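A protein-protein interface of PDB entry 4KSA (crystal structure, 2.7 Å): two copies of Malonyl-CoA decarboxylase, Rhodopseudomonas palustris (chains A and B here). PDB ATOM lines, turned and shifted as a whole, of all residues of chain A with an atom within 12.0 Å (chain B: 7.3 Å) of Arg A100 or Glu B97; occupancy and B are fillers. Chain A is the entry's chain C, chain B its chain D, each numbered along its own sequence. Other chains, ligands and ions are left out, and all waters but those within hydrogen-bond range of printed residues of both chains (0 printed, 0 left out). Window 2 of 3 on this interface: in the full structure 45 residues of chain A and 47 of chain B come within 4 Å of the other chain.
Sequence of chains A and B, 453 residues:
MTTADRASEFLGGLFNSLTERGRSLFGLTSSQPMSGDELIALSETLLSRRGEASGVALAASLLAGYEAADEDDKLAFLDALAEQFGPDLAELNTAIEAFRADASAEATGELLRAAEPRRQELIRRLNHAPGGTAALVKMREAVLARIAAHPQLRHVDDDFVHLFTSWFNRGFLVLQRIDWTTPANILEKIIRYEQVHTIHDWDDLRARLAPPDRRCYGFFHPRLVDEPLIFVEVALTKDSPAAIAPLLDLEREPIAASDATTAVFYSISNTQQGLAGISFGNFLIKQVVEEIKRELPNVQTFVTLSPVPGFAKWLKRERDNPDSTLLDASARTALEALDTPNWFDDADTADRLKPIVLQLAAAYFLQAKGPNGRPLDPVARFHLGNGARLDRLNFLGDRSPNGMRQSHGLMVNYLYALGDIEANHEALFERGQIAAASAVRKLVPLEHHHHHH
Leu A92 touches Phe B99, and with the chains exchanged Phe A99 touches Leu B92. Leu A92 touches Leu B111, but with the chains exchanged Leu A111 does not touch Leu B92 (4.2 Å). Asn A93 touches Arg B100, but with the chains exchanged Arg A100 does not touch Asn B93 (6.9 Å). Ile A96 touches Leu B111, but with the chains exchanged Leu A111 does not touch Ile B96 (4.2 Å). 13 positions are printed for both chains.
Of the 13 printed residues of chain B, 7 touch a printed residue of chain A. Printed residues of chain B that touch a printed residue of chain A: Leu B92, Asn B93, Ile B96, Glu B97, Phe B99, Arg B100 and Leu B111. Hydrophobic or aromatic side chains of chain B that line the printed part of chain A: Leu B92, Ile B96, Phe B99 and Leu B111. Of the 24 printed residues of chain A, 6 touch a printed residue of chain B. Printed residues of chain A that touch a printed residue of chain B: Leu A92, Asn A93, Ile A96, Glu A97, Phe A99 and Arg A100. Hydrophobic or aromatic side chains of chain A that line the printed part of chain B: Leu A92, Ile A96 and Phe A99. Among the printed residues, 11 pairs touch across the chains.
The backbone carbonyl oxygen of Leu A89 sits at hydrogen-bond distance from the side-chain amide nitrogen of Asn A93, at 3.3 Å. The side-chain carboxylate (OE1) of Glu A97 lies within salt-bridge range of the guanidinium group (NE) of Arg A100, 3.5 Å away.
Glu B97 touches just one residue of chain A: Arg A100 (3.4 Å). Asn B93 touches one residue of chain A. No residue of chain A comes within 4 Å of Thr B94. Ile B96 touches two residues of chain A. No residue of chain A comes within 4 Å of Ala B98. No residue of chain A comes within 4 Å of Ala B101. Printed residues of chain A within 4 Å of Phe B99: Leu A92 (3.7 Å). Of the printed residues of chain A, Leu B111 touches Leu A92 and Ile A96.
Leu A92 touches Phe B99 (CD2 to CZ, 3.7 Å). CD2 of Leu B111 touches CD1 of Leu A92 (3.7 Å). Asn A93 touches Arg B100. CG2 of Ile A96 touches CG2 of Ile B96 (3.4 Å). CD2 of Leu B111 touches CD1 of Ile A96, 3.4 Å away. Phe A99 touches Leu B92. Asn B93 touches Phe A99 (OD1 to CE1, 3.6 Å). Ile B96 touches Phe A99.
OE1 of Glu A97 lies within salt-bridge range of NH1 of Arg B100, 2.8 Å away. The side-chain carboxylate (OE2) of Glu B97 lies within salt-bridge range of the guanidinium group (NH1) of Arg A100. The guanidinium group of Arg B100 sits close to the guanidinium group of Arg A100 (3.3 Å).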
ATOM      1  N   LEU A  89     -30.740 -26.093  -5.637  1.00  0.00           N
ATOM      2  CA  LEU A  89     -29.718 -25.141  -5.196  1.00  0.00           C
ATOM      3  C   LEU A  89     -28.283 -25.676  -5.133  1.00  0.00           C
ATOM      4  O   LEU A  89     -27.337 -24.971  -5.496  1.00  0.00           O
ATOM      5  CB  LEU A  89     -30.103 -24.539  -3.836  1.00  0.00           C
ATOM      6  CG  LEU A  89     -31.415 -23.746  -3.707  1.00  0.00           C
ATOM      7  CD1 LEU A  89     -31.529 -22.691  -4.824  1.00  0.00           C
ATOM      8  CD2 LEU A  89     -32.590 -24.720  -3.756  1.00  0.00           C
ATOM      9  N   ALA A  90     -28.114 -26.910  -4.659  1.00  0.00           N
ATOM     10  CA  ALA A  90     -26.777 -27.494  -4.573  1.00  0.00           C
ATOM     11  C   ALA A  90     -26.194 -27.540  -5.976  1.00  0.00           C
ATOM     12  O   ALA A  90     -25.224 -26.833  -6.278  1.00  0.00           O
ATOM     13  CB  ALA A  90     -26.847 -28.892  -3.994  1.00  0.00           C
ATOM     14  N   GLU A  91     -26.808 -28.368  -6.824  1.00  0.00           N
ATOM     15  CA  GLU A  91     -26.387 -28.539  -8.210  1.00  0.00           C
ATOM     16  C   GLU A  91     -26.052 -27.200  -8.862  1.00  0.00           C
ATOM     17  O   GLU A  91     -24.993 -27.042  -9.479  1.00  0.00           O
ATOM     18  CB  GLU A  91     -27.496 -29.201  -9.027  1.00  0.00           C
ATOM     19  CG  GLU A  91     -28.104 -30.459  -8.435  1.00  0.00           C
ATOM     20  CD  GLU A  91     -27.481 -31.738  -8.977  1.00  0.00           C
ATOM     21  OE1 GLU A  91     -27.306 -31.838 -10.219  1.00  0.00           O
ATOM     22  OE2 GLU A  91     -27.183 -32.648  -8.163  1.00  0.00           O
ATOM     23  N   LEU A  92     -26.964 -26.241  -8.734  1.00  0.00           N
ATOM     24  CA  LEU A  92     -26.760 -24.943  -9.341  1.00  0.00           C
ATOM     25  C   LEU A  92     -25.485 -24.270  -8.842  1.00  0.00           C
ATOM     26  O   LEU A  92     -24.768 -23.647  -9.619  1.00  0.00           O
ATOM     27  CB  LEU A  92     -27.974 -24.046  -9.094  1.00  0.00           C
ATOM     28  CG  LEU A  92     -27.882 -22.610  -9.617  1.00  0.00           C
ATOM     29  CD1 LEU A  92     -27.642 -22.604 -11.119  1.00  0.00           C
ATOM     30  CD2 LEU A  92     -29.164 -21.871  -9.269  1.00  0.00           C
ATOM     31  N   ASN A  93     -25.196 -24.388  -7.552  1.00  0.00           N
ATOM     32  CA  ASN A  93     -23.981 -23.778  -7.021  1.00  0.00           C
ATOM     33  C   ASN A  93     -22.750 -24.483  -7.584  1.00  0.00           C
ATOM     34  O   ASN A  93     -21.828 -23.837  -8.112  1.00  0.00           O
ATOM     35  CB  ASN A  93     -23.981 -23.825  -5.497  1.00  0.00           C
ATOM     36  CG  ASN A  93     -24.411 -22.508  -4.894  1.00  0.00           C
ATOM     37  OD1 ASN A  93     -23.755 -21.479  -5.098  1.00  0.00           O
ATOM     38  ND2 ASN A  93     -25.526 -22.521  -4.163  1.00  0.00           N
ATOM     39  N   THR A  94     -22.738 -25.805  -7.461  1.00  0.00           N
ATOM     40  CA  THR A  94     -21.654 -26.605  -7.998  1.00  0.00           C
ATOM     41  C   THR A  94     -21.382 -26.073  -9.397  1.00  0.00           C
ATOM     42  O   THR A  94     -20.265 -25.688  -9.732  1.00  0.00           O
ATOM     43  CB  THR A  94     -22.074 -28.071  -8.151  1.00  0.00           C
ATOM     44  OG1 THR A  94     -22.517 -28.588  -6.890  1.00  0.00           O
ATOM     45  CG2 THR A  94     -20.923 -28.889  -8.656  1.00  0.00           C
ATOM     46  N   ALA A  95     -22.441 -26.051 -10.202  1.00  0.00           N
ATOM     47  CA  ALA A  95     -22.374 -25.597 -11.581  1.00  0.00           C
ATOM     48  C   ALA A  95     -21.870 -24.165 -11.723  1.00  0.00           C
ATOM     49  O   ALA A  95     -21.216 -23.840 -12.712  1.00  0.00           O
ATOM     50  CB  ALA A  95     -23.742 -25.751 -12.234  1.00  0.00           C
ATOM     51  N   ILE A  96     -22.177 -23.314 -10.746  1.00  0.00           N
ATOM     52  CA  ILE A  96     -21.726 -21.919 -10.769  1.00  0.00           C
ATOM     53  C   ILE A  96     -20.214 -21.862 -10.519  1.00  0.00           C
ATOM     54  O   ILE A  96     -19.481 -21.124 -11.188  1.00  0.00           O
ATOM     55  CB  ILE A  96     -22.410 -21.054  -9.663  1.00  0.00           C
ATOM     56  CG1 ILE A  96     -23.903 -20.884  -9.944  1.00  0.00           C
ATOM     57  CG2 ILE A  96     -21.756 -19.671  -9.602  1.00  0.00           C
ATOM     58  CD1 ILE A  96     -24.200 -19.882 -11.026  1.00  0.00           C
ATOM     59  N   GLU A  97     -19.748 -22.637  -9.545  1.00  0.00           N
ATOM     60  CA  GLU A  97     -18.332 -22.630  -9.233  1.00  0.00           C
ATOM     61  C   GLU A  97     -17.535 -23.070 -10.463  1.00  0.00           C
ATOM     62  O   GLU A  97     -16.552 -22.420 -10.839  1.00  0.00           O
ATOM     63  CB  GLU A  97     -18.045 -23.539  -8.034  1.00  0.00           C
ATOM     64  CG  GLU A  97     -16.665 -23.320  -7.429  1.00  0.00           C
ATOM     65  CD  GLU A  97     -16.538 -22.011  -6.650  1.00  0.00           C
ATOM     66  OE1 GLU A  97     -17.317 -21.051  -6.896  1.00  0.00           O
ATOM     67  OE2 GLU A  97     -15.630 -21.946  -5.792  1.00  0.00           O
ATOM     68  N   ALA A  98     -17.979 -24.153 -11.098  1.00  0.00           N
ATOM     69  CA  ALA A  98     -17.326 -24.678 -12.297  1.00  0.00           C
ATOM     70  C   ALA A  98     -17.202 -23.611 -13.385  1.00  0.00           C
ATOM     71  O   ALA A  98     -16.140 -23.439 -13.997  1.00  0.00           O
ATOM     72  CB  ALA A  98     -18.095 -25.868 -12.833  1.00  0.00           C
ATOM     73  N   PHE A  99     -18.283 -22.887 -13.637  1.00  0.00           N
ATOM     74  CA  PHE A  99     -18.210 -21.853 -14.654  1.00  0.00           C
ATOM     75  C   PHE A  99     -17.223 -20.779 -14.243  1.00  0.00           C
ATOM     76  O   PHE A  99     -16.448 -20.296 -15.059  1.00  0.00           O
ATOM     77  CB  PHE A  99     -19.577 -21.228 -14.894  1.00  0.00           C
ATOM     78  CG  PHE A  99     -19.537 -20.068 -15.822  1.00  0.00           C
ATOM     79  CD1 PHE A  99     -19.356 -18.778 -15.336  1.00  0.00           C
ATOM     80  CD2 PHE A  99     -19.667 -20.258 -17.190  1.00  0.00           C
ATOM     81  CE1 PHE A  99     -19.306 -17.680 -16.205  1.00  0.00           C
ATOM     82  CE2 PHE A  99     -19.618 -19.170 -18.071  1.00  0.00           C
ATOM     83  CZ  PHE A  99     -19.437 -17.876 -17.573  1.00  0.00           C
ATOM     84  N   ARG A 100     -17.268 -20.401 -12.968  1.00  0.00           N
ATOM     85  CA  ARG A 100     -16.375 -19.385 -12.431  1.00  0.00           C
ATOM     86  C   ARG A 100     -14.907 -19.818 -12.567  1.00  0.00           C
ATOM     87  O   ARG A 100     -14.020 -18.981 -12.763  1.00  0.00           O
ATOM     88  CB  ARG A 100     -16.706 -19.135 -10.961  1.00  0.00           C
ATOM     89  CG  ARG A 100     -17.998 -18.367 -10.705  1.00  0.00           C
ATOM     90  CD  ARG A 100     -18.330 -18.365  -9.214  1.00  0.00           C
ATOM     91  NE  ARG A 100     -17.201 -17.917  -8.400  1.00  0.00           N
ATOM     92  CZ  ARG A 100     -16.657 -16.709  -8.495  1.00  0.00           C
ATOM     93  NH1 ARG A 100     -17.147 -15.829  -9.363  1.00  0.00           N
ATOM     94  NH2 ARG A 100     -15.604 -16.387  -7.753  1.00  0.00           N
ATOM     95  N   ALA A 101     -14.660 -21.124 -12.465  1.00  0.00           N
ATOM     96  CA  ALA A 101     -13.310 -21.667 -12.584  1.00  0.00           C
ATOM     97  C   ALA A 101     -12.834 -21.698 -14.050  1.00  0.00           C
ATOM     98  O   ALA A 101     -11.678 -21.383 -14.355  1.00  0.00           O
ATOM     99  CB  ALA A 101     -13.272 -23.062 -11.986  1.00  0.00           C
ATOM    100  N   ASP A 102     -13.731 -22.073 -14.957  1.00  0.00           N
ATOM    101  CA  ASP A 102     -13.402 -22.148 -16.375  1.00  0.00           C
ATOM    102  C   ASP A 102     -14.678 -21.963 -17.203  1.00  0.00           C
ATOM    103  O   ASP A 102     -15.534 -22.847 -17.228  1.00  0.00           O
ATOM    104  CB  ASP A 102     -12.772 -23.516 -16.676  1.00  0.00           C
ATOM    105  CG  ASP A 102     -12.404 -23.700 -18.152  1.00  0.00           C
ATOM    106  OD1 ASP A 102     -12.098 -24.858 -18.536  1.00  0.00           O
ATOM    107  OD2 ASP A 102     -12.411 -22.704 -18.916  1.00  0.00           O
ATOM    108  N   ALA A 103     -14.805 -20.815 -17.871  1.00  0.00           N
ATOM    109  CA  ALA A 103     -15.980 -20.541 -18.697  1.00  0.00           C
ATOM    110  C   ALA A 103     -15.981 -21.418 -19.952  1.00  0.00           C
ATOM    111  O   ALA A 103     -15.959 -20.911 -21.069  1.00  0.00           O
ATOM    112  CB  ALA A 103     -16.024 -19.067 -19.090  1.00  0.00           C
ATOM    113  N   SER A 104     -16.008 -22.732 -19.752  1.00  0.00           N
ATOM    114  CA  SER A 104     -16.008 -23.686 -20.851  1.00  0.00           C
ATOM    115  C   SER A 104     -17.433 -24.027 -21.326  1.00  0.00           C
ATOM    116  O   SER A 104     -18.421 -23.632 -20.696  1.00  0.00           O
ATOM    117  CB  SER A 104     -15.300 -24.970 -20.414  1.00  0.00           C
ATOM    118  OG  SER A 104     -16.096 -25.737 -19.533  1.00  0.00           O
ATOM    119  N   ALA A 105     -17.531 -24.759 -22.437  1.00  0.00           N
ATOM    120  CA  ALA A 105     -18.821 -25.171 -22.984  1.00  0.00           C
ATOM    121  C   ALA A 105     -19.471 -26.159 -22.030  1.00  0.00           C
ATOM    122  O   ALA A 105     -20.652 -26.038 -21.716  1.00  0.00           O
ATOM    123  CB  ALA A 105     -18.639 -25.807 -24.341  1.00  0.00           C
ATOM    124  N   GLU A 106     -18.699 -27.134 -21.557  1.00  0.00           N
ATOM    125  CA  GLU A 106     -19.238 -28.123 -20.625  1.00  0.00           C
ATOM    126  C   GLU A 106     -19.871 -27.409 -19.432  1.00  0.00           C
ATOM    127  O   GLU A 106     -20.990 -27.723 -19.038  1.00  0.00           O
ATOM    128  CB  GLU A 106     -18.140 -29.071 -20.110  1.00  0.00           C
ATOM    129  CG  GLU A 106     -18.686 -30.430 -19.634  1.00  0.00           C
ATOM    130  CD  GLU A 106     -17.906 -31.053 -18.462  1.00  0.00           C
ATOM    131  OE1 GLU A 106     -18.023 -32.284 -18.258  1.00  0.00           O
ATOM    132  OE2 GLU A 106     -17.195 -30.324 -17.730  1.00  0.00           O
ATOM    133  N   ALA A 107     -19.153 -26.437 -18.874  1.00  0.00           N
ATOM    134  CA  ALA A 107     -19.632 -25.695 -17.706  1.00  0.00           C
ATOM    135  C   ALA A 107     -20.810 -24.761 -17.979  1.00  0.00           C
ATOM    136  O   ALA A 107     -21.668 -24.564 -17.115  1.00  0.00           O
ATOM    137  CB  ALA A 107     -18.482 -24.900 -17.088  1.00  0.00           C
ATOM    138  N   THR A 108     -20.840 -24.187 -19.175  1.00  0.00           N
ATOM    139  CA  THR A 108     -21.903 -23.274 -19.546  1.00  0.00           C
ATOM    140  C   THR A 108     -23.175 -24.043 -19.907  1.00  0.00           C
ATOM    141  O   THR A 108     -24.260 -23.477 -19.966  1.00  0.00           O
ATOM    142  CB  THR A 108     -21.472 -22.392 -20.722  1.00  0.00           C
ATOM    143  OG1 THR A 108     -22.524 -21.489 -21.051  1.00  0.00           O
ATOM    144  CG2 THR A 108     -21.169 -23.232 -21.927  1.00  0.00           C
ATOM    145  N   GLY A 109     -23.040 -25.340 -20.139  1.00  0.00           N
ATOM    146  CA  GLY A 109     -24.199 -26.146 -20.466  1.00  0.00           C
ATOM    147  C   GLY A 109     -24.846 -26.715 -19.220  1.00  0.00           C
ATOM    148  O   GLY A 109     -26.073 -26.749 -19.110  1.00  0.00           O
ATOM    149  N   GLU A 110     -24.021 -27.172 -18.281  1.00  0.00           N
ATOM    150  CA  GLU A 110     -24.514 -27.727 -17.027  1.00  0.00           C
ATOM    151  C   GLU A 110     -25.178 -26.621 -16.229  1.00  0.00           C
ATOM    152  O   GLU A 110     -26.079 -26.875 -15.433  1.00  0.00           O
ATOM    153  CB  GLU A 110     -23.369 -28.299 -16.201  1.00  0.00           C
ATOM    154  CG  GLU A 110     -23.798 -28.879 -14.862  1.00  0.00           C
ATOM    155  CD  GLU A 110     -24.811 -30.005 -15.010  1.00  0.00           C
ATOM    156  OE1 GLU A 110     -26.027 -29.720 -15.092  1.00  0.00           O
ATOM    157  OE2 GLU A 110     -24.390 -31.186 -15.060  1.00  0.00           O
ATOM    158  N   LEU A 111     -24.712 -25.392 -16.442  1.00  0.00           N
ATOM    159  CA  LEU A 111     -25.258 -24.231 -15.750  1.00  0.00           C
ATOM    160  C   LEU A 111     -26.677 -24.003 -16.279  1.00  0.00           C
ATOM    161  O   LEU A 111     -27.606 -23.761 -15.517  1.00  0.00           O
ATOM    162  CB  LEU A 111     -24.376 -23.009 -16.001  1.00  0.00           C
ATOM    163  CG  LEU A 111     -24.222 -22.020 -14.846  1.00  0.00           C
ATOM    164  CD1 LEU A 111     -23.287 -20.867 -15.241  1.00  0.00           C
ATOM    165  CD2 LEU A 111     -25.585 -21.493 -14.473  1.00  0.00           C
ATOM    166  N   LEU A 112     -26.843 -24.098 -17.590  1.00  0.00           N
ATOM    167  CA  LEU A 112     -28.158 -23.949 -18.193  1.00  0.00           C
ATOM    168  C   LEU A 112     -29.051 -25.065 -17.644  1.00  0.00           C
ATOM    169  O   LEU A 112     -30.201 -24.834 -17.320  1.00  0.00           O
ATOM    170  CB  LEU A 112     -28.060 -24.053 -19.720  1.00  0.00           C
ATOM    171  CG  LEU A 112     -29.367 -24.021 -20.522  1.00  0.00           C
ATOM    172  CD1 LEU A 112     -30.111 -22.726 -20.247  1.00  0.00           C
ATOM    173  CD2 LEU A 112     -29.054 -24.161 -22.007  1.00  0.00           C
ATOM    174  N   GLU B  91     -23.525 -10.705 -19.663  1.00  0.00           N
ATOM    175  CA  GLU B  91     -24.799 -10.819 -18.969  1.00  0.00           C
ATOM    176  C   GLU B  91     -24.853 -12.052 -18.051  1.00  0.00           C
ATOM    177  O   GLU B  91     -25.523 -12.040 -17.017  1.00  0.00           O
ATOM    178  CB  GLU B  91     -25.934 -10.846 -19.999  1.00  0.00           C
ATOM    179  CG  GLU B  91     -27.335 -11.043 -19.419  1.00  0.00           C
ATOM    180  CD  GLU B  91     -28.432 -10.995 -20.485  1.00  0.00           C
ATOM    181  OE1 GLU B  91     -29.563 -11.462 -20.200  1.00  0.00           O
ATOM    182  OE2 GLU B  91     -28.166 -10.480 -21.600  1.00  0.00           O
ATOM    183  N   LEU B  92     -24.147 -13.114 -18.413  1.00  0.00           N
ATOM    184  CA  LEU B  92     -24.156 -14.296 -17.567  1.00  0.00           C
ATOM    185  C   LEU B  92     -23.422 -13.943 -16.279  1.00  0.00           C
ATOM    186  O   LEU B  92     -23.868 -14.289 -15.185  1.00  0.00           O
ATOM    187  CB  LEU B  92     -23.439 -15.467 -18.247  1.00  0.00           C
ATOM    188  CG  LEU B  92     -23.955 -16.894 -18.012  1.00  0.00           C
ATOM    189  CD1 LEU B  92     -22.829 -17.857 -18.282  1.00  0.00           C
ATOM    190  CD2 LEU B  92     -24.469 -17.094 -16.606  1.00  0.00           C
ATOM    191  N   ASN B  93     -22.294 -13.246 -16.421  1.00  0.00           N
ATOM    192  CA  ASN B  93     -21.468 -12.853 -15.279  1.00  0.00           C
ATOM    193  C   ASN B  93     -22.227 -11.996 -14.275  1.00  0.00           C
ATOM    194  O   ASN B  93     -22.178 -12.227 -13.059  1.00  0.00           O
ATOM    195  CB  ASN B  93     -20.230 -12.101 -15.761  1.00  0.00           C
ATOM    196  CG  ASN B  93     -19.268 -12.991 -16.525  1.00  0.00           C
ATOM    197  OD1 ASN B  93     -18.939 -14.091 -16.078  1.00  0.00           O
ATOM    198  ND2 ASN B  93     -18.801 -12.517 -17.677  1.00  0.00           N
ATOM    199  N   THR B  94     -22.931 -10.999 -14.783  1.00  0.00           N
ATOM    200  CA  THR B  94     -23.701 -10.145 -13.909  1.00  0.00           C
ATOM    201  C   THR B  94     -24.707 -11.024 -13.160  1.00  0.00           C
ATOM    202  O   THR B  94     -24.785 -10.990 -11.930  1.00  0.00           O
ATOM    203  CB  THR B  94     -24.465  -9.086 -14.712  1.00  0.00           C
ATOM    204  OG1 THR B  94     -23.564  -8.423 -15.611  1.00  0.00           O
ATOM    205  CG2 THR B  94     -25.112  -8.072 -13.767  1.00  0.00           C
ATOM    206  N   ALA B  95     -25.459 -11.826 -13.912  1.00  0.00           N
ATOM    207  CA  ALA B  95     -26.469 -12.699 -13.330  1.00  0.00           C
ATOM    208  C   ALA B  95     -25.912 -13.590 -12.236  1.00  0.00           C
ATOM    209  O   ALA B  95     -26.604 -13.870 -11.258  1.00  0.00           O
ATOM    210  CB  ALA B  95     -27.112 -13.547 -14.414  1.00  0.00           C
ATOM    211  N   ILE B  96     -24.666 -14.033 -12.406  1.00  0.00           N
ATOM    212  CA  ILE B  96     -24.009 -14.891 -11.418  1.00  0.00           C
ATOM    213  C   ILE B  96     -23.580 -14.062 -10.207  1.00  0.00           C
ATOM    214  O   ILE B  96     -23.763 -14.479  -9.060  1.00  0.00           O
ATOM    215  CB  ILE B  96     -22.752 -15.592 -12.000  1.00  0.00           C
ATOM    216  CG1 ILE B  96     -23.101 -16.303 -13.309  1.00  0.00           C
ATOM    217  CG2 ILE B  96     -22.238 -16.629 -11.018  1.00  0.00           C
ATOM    218  CD1 ILE B  96     -21.969 -17.121 -13.896  1.00  0.00           C
ATOM    219  N   GLU B  97     -23.004 -12.890 -10.454  1.00  0.00           N
ATOM    220  CA  GLU B  97     -22.586 -12.053  -9.342  1.00  0.00           C
ATOM    221  C   GLU B  97     -23.813 -11.669  -8.528  1.00  0.00           C
ATOM    222  O   GLU B  97     -23.766 -11.640  -7.300  1.00  0.00           O
ATOM    223  CB  GLU B  97     -21.846 -10.808  -9.837  1.00  0.00           C
ATOM    224  CG  GLU B  97     -20.431 -11.102 -10.351  1.00  0.00           C
ATOM    225  CD  GLU B  97     -19.613 -12.009  -9.408  1.00  0.00           C
ATOM    226  OE1 GLU B  97     -19.460 -11.659  -8.212  1.00  0.00           O
ATOM    227  OE2 GLU B  97     -19.119 -13.073  -9.868  1.00  0.00           O
ATOM    228  N   ALA B  98     -24.918 -11.401  -9.219  1.00  0.00           N
ATOM    229  CA  ALA B  98     -26.177 -11.048  -8.571  1.00  0.00           C
ATOM    230  C   ALA B  98     -26.690 -12.214  -7.710  1.00  0.00           C
ATOM    231  O   ALA B  98     -27.152 -12.017  -6.580  1.00  0.00           O
ATOM    232  CB  ALA B  98     -27.200 -10.684  -9.624  1.00  0.00           C
ATOM    233  N   PHE B  99     -26.603 -13.427  -8.252  1.00  0.00           N
ATOM    234  CA  PHE B  99     -27.051 -14.624  -7.541  1.00  0.00           C
ATOM    235  C   PHE B  99     -26.152 -14.893  -6.346  1.00  0.00           C
ATOM    236  O   PHE B  99     -26.629 -15.209  -5.268  1.00  0.00           O
ATOM    237  CB  PHE B  99     -27.071 -15.839  -8.486  1.00  0.00           C
ATOM    238  CG  PHE B  99     -27.454 -17.144  -7.816  1.00  0.00           C
ATOM    239  CD1 PHE B  99     -26.482 -17.986  -7.294  1.00  0.00           C
ATOM    240  CD2 PHE B  99     -28.786 -17.531  -7.716  1.00  0.00           C
ATOM    241  CE1 PHE B  99     -26.827 -19.194  -6.687  1.00  0.00           C
ATOM    242  CE2 PHE B  99     -29.138 -18.741  -7.109  1.00  0.00           C
ATOM    243  CZ  PHE B  99     -28.152 -19.572  -6.593  1.00  0.00           C
ATOM    244  N   ARG B 100     -24.845 -14.777  -6.534  1.00  0.00           N
ATOM    245  CA  ARG B 100     -23.926 -14.997  -5.422  1.00  0.00           C
ATOM    246  C   ARG B 100     -24.277 -14.048  -4.265  1.00  0.00           C
ATOM    247  O   ARG B 100     -24.362 -14.468  -3.097  1.00  0.00           O
ATOM    248  CB  ARG B 100     -22.482 -14.763  -5.863  1.00  0.00           C
ATOM    249  CG  ARG B 100     -21.822 -15.985  -6.440  1.00  0.00           C
ATOM    250  CD  ARG B 100     -20.326 -15.960  -6.165  1.00  0.00           C
ATOM    251  NE  ARG B 100     -19.725 -17.261  -6.439  1.00  0.00           N
ATOM    252  CZ  ARG B 100     -20.149 -18.411  -5.915  1.00  0.00           C
ATOM    253  NH1 ARG B 100     -19.537 -19.550  -6.230  1.00  0.00           N
ATOM    254  NH2 ARG B 100     -21.181 -18.426  -5.076  1.00  0.00           N
ATOM    255  N   ALA B 101     -24.477 -12.777  -4.614  1.00  0.00           N
ATOM    256  CA  ALA B 101     -24.834 -11.736  -3.662  1.00  0.00           C
ATOM    257  C   ALA B 101     -26.145 -12.081  -2.963  1.00  0.00           C
ATOM    258  O   ALA B 101     -26.218 -12.126  -1.738  1.00  0.00           O
ATOM    259  CB  ALA B 101     -24.967 -10.409  -4.381  1.00  0.00           C
ATOM    260  N   ASP B 102     -27.186 -12.330  -3.749  1.00  0.00           N
ATOM    261  CA  ASP B 102     -28.480 -12.677  -3.181  1.00  0.00           C
ATOM    262  C   ASP B 102     -29.130 -13.798  -3.991  1.00  0.00           C
ATOM    263  O   ASP B 102     -29.653 -13.554  -5.080  1.00  0.00           O
ATOM    264  CB  ASP B 102     -29.377 -11.437  -3.162  1.00  0.00           C
ATOM    265  CG  ASP B 102     -30.776 -11.741  -2.663  1.00  0.00           C
ATOM    266  OD1 ASP B 102     -30.906 -12.440  -1.628  1.00  0.00           O
ATOM    267  OD2 ASP B 102     -31.741 -11.272  -3.303  1.00  0.00           O
ATOM    268  N   LEU B 111     -30.608 -15.977 -13.722  1.00  0.00           N
ATOM    269  CA  LEU B 111     -29.465 -16.804 -14.051  1.00  0.00           C
ATOM    270  C   LEU B 111     -29.826 -17.772 -15.180  1.00  0.00           C
ATOM    271  O   LEU B 111     -29.028 -18.007 -16.089  1.00  0.00           O
ATOM    272  CB  LEU B 111     -29.020 -17.566 -12.801  1.00  0.00           C
ATOM    273  CG  LEU B 111     -27.715 -18.363 -12.825  1.00  0.00           C
ATOM    274  CD1 LEU B 111     -26.559 -17.508 -13.332  1.00  0.00           C
ATOM    275  CD2 LEU B 111     -27.448 -18.876 -11.426  1.00  0.00           C
